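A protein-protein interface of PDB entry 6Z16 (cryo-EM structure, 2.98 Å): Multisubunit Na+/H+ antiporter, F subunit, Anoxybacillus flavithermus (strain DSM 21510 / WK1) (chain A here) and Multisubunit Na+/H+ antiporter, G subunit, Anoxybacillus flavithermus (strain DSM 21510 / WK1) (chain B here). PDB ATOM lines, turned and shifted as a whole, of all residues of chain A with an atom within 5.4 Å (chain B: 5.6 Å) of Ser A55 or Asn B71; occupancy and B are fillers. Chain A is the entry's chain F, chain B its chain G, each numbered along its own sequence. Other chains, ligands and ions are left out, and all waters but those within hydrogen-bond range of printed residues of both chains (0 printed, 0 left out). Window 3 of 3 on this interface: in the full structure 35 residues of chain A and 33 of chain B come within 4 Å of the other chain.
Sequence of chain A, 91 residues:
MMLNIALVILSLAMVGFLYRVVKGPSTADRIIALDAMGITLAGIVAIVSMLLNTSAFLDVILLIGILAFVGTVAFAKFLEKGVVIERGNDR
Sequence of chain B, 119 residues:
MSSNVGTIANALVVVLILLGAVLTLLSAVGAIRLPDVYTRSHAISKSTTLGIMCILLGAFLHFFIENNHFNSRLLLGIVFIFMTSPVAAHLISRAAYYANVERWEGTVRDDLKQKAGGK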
ATOM      1  N   ASN A  53       0.203  -3.483  15.664  1.00  0.00           N
ATOM      2  CA  ASN A  53       0.370  -3.029  17.051  1.00  0.00           C
ATOM      3  C   ASN A  53       1.698  -2.295  17.230  1.00  0.00           C
ATOM      4  O   ASN A  53       2.431  -2.512  18.195  1.00  0.00           O
ATOM      5  CB  ASN A  53       0.227  -4.191  18.043  1.00  0.00           C
ATOM      6  CG  ASN A  53      -0.077  -3.728  19.452  1.00  0.00           C
ATOM      7  OD1 ASN A  53      -0.180  -2.533  19.715  1.00  0.00           O
ATOM      8  ND2 ASN A  53      -0.222  -4.676  20.368  1.00  0.00           N
ATOM      9  N   THR A  54       2.024  -1.433  16.273  1.00  0.00           N
ATOM     10  CA  THR A  54       3.248  -0.650  16.317  1.00  0.00           C
ATOM     11  C   THR A  54       2.931   0.811  16.052  1.00  0.00           C
ATOM     12  O   THR A  54       2.078   1.141  15.225  1.00  0.00           O
ATOM     13  CB  THR A  54       4.294  -1.125  15.286  1.00  0.00           C
ATOM     14  OG1 THR A  54       3.757  -1.023  13.962  1.00  0.00           O
ATOM     15  CG2 THR A  54       4.735  -2.557  15.553  1.00  0.00           C
ATOM     16  N   SER A  55       3.644   1.685  16.755  1.00  0.00           N
ATOM     17  CA  SER A  55       3.577   3.121  16.530  1.00  0.00           C
ATOM     18  C   SER A  55       4.710   3.609  15.635  1.00  0.00           C
ATOM     19  O   SER A  55       5.178   4.740  15.787  1.00  0.00           O
ATOM     20  CB  SER A  55       3.607   3.864  17.864  1.00  0.00           C
ATOM     21  OG  SER A  55       2.492   3.524  18.667  1.00  0.00           O
ATOM     22  N   ALA A  56       5.159   2.776  14.703  1.00  0.00           N
ATOM     23  CA  ALA A  56       6.375   3.036  13.950  1.00  0.00           C
ATOM     24  C   ALA A  56       6.117   3.519  12.533  1.00  0.00           C
ATOM     25  O   ALA A  56       7.053   3.563  11.733  1.00  0.00           O
ATOM     26  CB  ALA A  56       7.243   1.779  13.917  1.00  0.00           C
ATOM     27  N   PHE A  57       4.880   3.890  12.197  1.00  0.00           N
ATOM     28  CA  PHE A  57       4.556   4.229  10.816  1.00  0.00           C
ATOM     29  C   PHE A  57       3.717   5.496  10.693  1.00  0.00           C
ATOM     30  O   PHE A  57       3.128   5.727   9.638  1.00  0.00           O
ATOM     31  CB  PHE A  57       3.821   3.073  10.133  1.00  0.00           C
ATOM     32  CG  PHE A  57       4.633   1.819  10.006  1.00  0.00           C
ATOM     33  CD1 PHE A  57       5.563   1.674   8.992  1.00  0.00           C
ATOM     34  CD2 PHE A  57       4.456   0.777  10.899  1.00  0.00           C
ATOM     35  CE1 PHE A  57       6.307   0.516   8.876  1.00  0.00           C
ATOM     36  CE2 PHE A  57       5.195  -0.379  10.791  1.00  0.00           C
ATOM     37  CZ  PHE A  57       6.121  -0.511   9.779  1.00  0.00           C
ATOM     38  N   LEU A  58       3.630   6.320  11.738  1.00  0.00           N
ATOM     39  CA  LEU A  58       2.765   7.494  11.657  1.00  0.00           C
ATOM     40  C   LEU A  58       3.430   8.611  10.860  1.00  0.00           C
ATOM     41  O   LEU A  58       2.745   9.439  10.227  1.00  0.00           O
ATOM     42  CB  LEU A  58       2.407   8.004  13.054  1.00  0.00           C
ATOM     43  CG  LEU A  58       1.558   7.135  13.996  1.00  0.00           C
ATOM     44  CD1 LEU A  58       0.417   6.424  13.300  1.00  0.00           C
ATOM     45  CD2 LEU A  58       2.371   6.172  14.817  1.00  0.00           C
ATOM     46  N   PHE B  60      -5.552   7.374  16.484  1.00  0.00           N
ATOM     47  CA  PHE B  60      -5.047   8.202  17.573  1.00  0.00           C
ATOM     48  C   PHE B  60      -5.628   7.785  18.916  1.00  0.00           C
ATOM     49  O   PHE B  60      -4.888   7.571  19.885  1.00  0.00           O
ATOM     50  CB  PHE B  60      -5.366   9.663  17.263  1.00  0.00           C
ATOM     51  CG  PHE B  60      -5.067  10.597  18.378  1.00  0.00           C
ATOM     52  CD1 PHE B  60      -3.762  10.910  18.703  1.00  0.00           C
ATOM     53  CD2 PHE B  60      -6.098  11.180  19.095  1.00  0.00           C
ATOM     54  CE1 PHE B  60      -3.489  11.770  19.739  1.00  0.00           C
ATOM     55  CE2 PHE B  60      -5.834  12.045  20.130  1.00  0.00           C
ATOM     56  CZ  PHE B  60      -4.529  12.341  20.454  1.00  0.00           C
ATOM     57  N   PHE B  63      -4.292   4.088  19.993  1.00  0.00           N
ATOM     58  CA  PHE B  63      -2.966   4.064  20.606  1.00  0.00           C
ATOM     59  C   PHE B  63      -2.922   4.865  21.897  1.00  0.00           C
ATOM     60  O   PHE B  63      -2.115   4.557  22.781  1.00  0.00           O
ATOM     61  CB  PHE B  63      -1.898   4.578  19.647  1.00  0.00           C
ATOM     62  CG  PHE B  63      -1.599   3.640  18.525  1.00  0.00           C
ATOM     63  CD1 PHE B  63      -0.954   2.441  18.774  1.00  0.00           C
ATOM     64  CD2 PHE B  63      -1.914   3.973  17.221  1.00  0.00           C
ATOM     65  CE1 PHE B  63      -0.671   1.573  17.749  1.00  0.00           C
ATOM     66  CE2 PHE B  63      -1.625   3.112  16.189  1.00  0.00           C
ATOM     67  CZ  PHE B  63      -1.004   1.908  16.456  1.00  0.00           C
ATOM     68  N   ASN B  67      -2.382   1.706  24.799  1.00  0.00           N
ATOM     69  CA  ASN B  67      -0.939   1.719  24.973  1.00  0.00           C
ATOM     70  C   ASN B  67      -0.447   2.827  25.886  1.00  0.00           C
ATOM     71  O   ASN B  67       0.724   2.787  26.277  1.00  0.00           O
ATOM     72  CB  ASN B  67      -0.228   1.840  23.616  1.00  0.00           C
ATOM     73  CG  ASN B  67      -0.499   0.658  22.709  1.00  0.00           C
ATOM     74  OD1 ASN B  67      -1.063   0.807  21.628  1.00  0.00           O
ATOM     75  ND2 ASN B  67      -0.117  -0.530  23.157  1.00  0.00           N
ATOM     76  N   HIS B  69       0.121   5.896  25.066  1.00  0.00           N
ATOM     77  CA  HIS B  69       1.130   6.597  24.286  1.00  0.00           C
ATOM     78  C   HIS B  69       0.452   7.725  23.528  1.00  0.00           C
ATOM     79  O   HIS B  69      -0.418   7.476  22.687  1.00  0.00           O
ATOM     80  CB  HIS B  69       1.839   5.651  23.312  1.00  0.00           C
ATOM     81  CG  HIS B  69       2.722   4.640  23.976  1.00  0.00           C
ATOM     82  ND1 HIS B  69       3.289   3.586  23.292  1.00  0.00           N
ATOM     83  CD2 HIS B  69       3.140   4.522  25.259  1.00  0.00           C
ATOM     84  CE1 HIS B  69       4.013   2.860  24.125  1.00  0.00           C
ATOM     85  NE2 HIS B  69       3.939   3.407  25.324  1.00  0.00           N
ATOM     86  N   PHE B  70       0.843   8.957  23.822  1.00  0.00           N
ATOM     87  CA  PHE B  70       0.257  10.125  23.179  1.00  0.00           C
ATOM     88  C   PHE B  70       1.051  10.427  21.916  1.00  0.00           C
ATOM     89  O   PHE B  70       2.196  10.885  21.989  1.00  0.00           O
ATOM     90  CB  PHE B  70       0.258  11.314  24.131  1.00  0.00           C
ATOM     91  CG  PHE B  70      -0.501  12.494  23.620  1.00  0.00           C
ATOM     92  CD1 PHE B  70      -1.884  12.510  23.667  1.00  0.00           C
ATOM     93  CD2 PHE B  70       0.161  13.585  23.091  1.00  0.00           C
ATOM     94  CE1 PHE B  70      -2.594  13.595  23.199  1.00  0.00           C
ATOM     95  CE2 PHE B  70      -0.542  14.671  22.618  1.00  0.00           C
ATOM     96  CZ  PHE B  70      -1.921  14.678  22.673  1.00  0.00           C
ATOM     97  N   ASN B  71       0.449  10.175  20.758  1.00  0.00           N
ATOM     98  CA  ASN B  71       1.119  10.342  19.470  1.00  0.00           C
ATOM     99  C   ASN B  71       0.603  11.617  18.816  1.00  0.00           C
ATOM    100  O   ASN B  71      -0.505  11.647  18.278  1.00  0.00           O
ATOM    101  CB  ASN B  71       0.889   9.123  18.585  1.00  0.00           C
ATOM    102  CG  ASN B  71       1.626   7.900  19.083  1.00  0.00           C
ATOM    103  OD1 ASN B  71       2.781   7.982  19.497  1.00  0.00           O
ATOM    104  ND2 ASN B  71       0.959   6.757  19.052  1.00  0.00           N
ATOM    105  N   SER B  72       1.420  12.667  18.849  1.00  0.00           N
ATOM    106  CA  SER B  72       1.020  13.962  18.322  1.00  0.00           C
ATOM    107  C   SER B  72       1.139  14.048  16.808  1.00  0.00           C
ATOM    108  O   SER B  72       0.579  14.978  16.206  1.00  0.00           O
ATOM    109  CB  SER B  72       1.867  15.058  18.961  1.00  0.00           C
ATOM    110  OG  SER B  72       1.693  15.073  20.363  1.00  0.00           O
ATOM    111  N   ARG B  73       1.857  13.101  16.192  1.00  0.00           N
ATOM    112  CA  ARG B  73       2.029  13.094  14.741  1.00  0.00           C
ATOM    113  C   ARG B  73       0.697  12.899  14.031  1.00  0.00           C
ATOM    114  O   ARG B  73       0.464  13.488  12.970  1.00  0.00           O
ATOM    115  CB  ARG B  73       2.998  11.986  14.315  1.00  0.00           C
ATOM    116  CG  ARG B  73       4.491  12.299  14.429  1.00  0.00           C
ATOM    117  CD  ARG B  73       4.998  12.135  15.853  1.00  0.00           C
ATOM    118  NE  ARG B  73       6.443  12.291  15.962  1.00  0.00           N
ATOM    119  CZ  ARG B  73       7.102  12.282  17.115  1.00  0.00           C
ATOM    120  NH1 ARG B  73       6.441  12.117  18.252  1.00  0.00           N
ATOM    121  NH2 ARG B  73       8.419  12.435  17.135  1.00  0.00           N
ATOM    122  N   LEU B  74      -0.197  12.106  14.626  1.00  0.00           N
ATOM    123  CA  LEU B  74      -1.528  11.907  14.066  1.00  0.00           C
ATOM    124  C   LEU B  74      -2.361  13.175  14.130  1.00  0.00           C
ATOM    125  O   LEU B  74      -3.099  13.479  13.188  1.00  0.00           O
ATOM    126  CB  LEU B  74      -2.229  10.774  14.800  1.00  0.00           C
ATOM    127  CG  LEU B  74      -1.658   9.422  14.414  1.00  0.00           C
ATOM    128  CD1 LEU B  74      -2.134   8.327  15.334  1.00  0.00           C
ATOM    129  CD2 LEU B  74      -2.095   9.137  12.997  1.00  0.00           C
ATOM    130  N   LEU B  75      -2.252  13.930  15.223  1.00  0.00           N
ATOM    131  CA  LEU B  75      -3.003  15.176  15.339  1.00  0.00           C
ATOM    132  C   LEU B  75      -2.507  16.209  14.340  1.00  0.00           C
ATOM    133  O   LEU B  75      -3.310  16.923  13.721  1.00  0.00           O
ATOM    134  CB  LEU B  75      -2.891  15.719  16.756  1.00  0.00           C
ATOM    135  CG  LEU B  75      -3.462  14.828  17.851  1.00  0.00           C
ATOM    136  CD1 LEU B  75      -3.216  15.460  19.200  1.00  0.00           C
ATOM    137  CD2 LEU B  75      -4.940  14.571  17.627  1.00  0.00           C
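Of the 10 printed residues of chain B, 4 touch a printed residue of chain A. Of the 6 printed residues of chain A, 4 touch a printed residue of chain B. Printed residues of chain A that touch a printed residue of chain B: Asn A53, Thr A54, Ser A55 and Leu A58. Hydrophobic or aromatic side chains of chain A within 4 Å of the printed part of chain B: Leu A58. Among the printed residues, no Asp or Glu carboxylate lies within 4 Å of a Lys or Arg side-chain nitrogen of the other chain.
Printed residues of chain B within 4 Å of Thr A54: Phe B63 (3.4 Å). Ser A55 touches just these residues of chain B: Phe B63 (3.6 Å) and Asn B71 (3.6 Å). Printed residues of chain A within 4 Å of Asn B67: Asn A53 (3.9 Å). Of chain A, only Ser A55 (3.6 Å) comes within 4 Å of Asn B71. Of the printed residues of chain A, Leu B74 touches Leu A58. Leu B75 touches none of the printed residues of chain A.
Among the printed residues, pairs that only touch across the chains: Asn A53 with Asn B67, Thr A54 with Phe B63, Ser A55 with Phe B63, Ser A55 with Asn B71 and Leu A58 with Leu B74.
The backbone carbonyl oxygen (O) of Phe B63 lies within hydrogen-bond range of the backbone NH (N) of His B69, at 3.5 Å. A ring nitrogen (NE2) of His B69 sits close to the backbone carbonyl oxygen of Asn B67 (3.4 Å).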
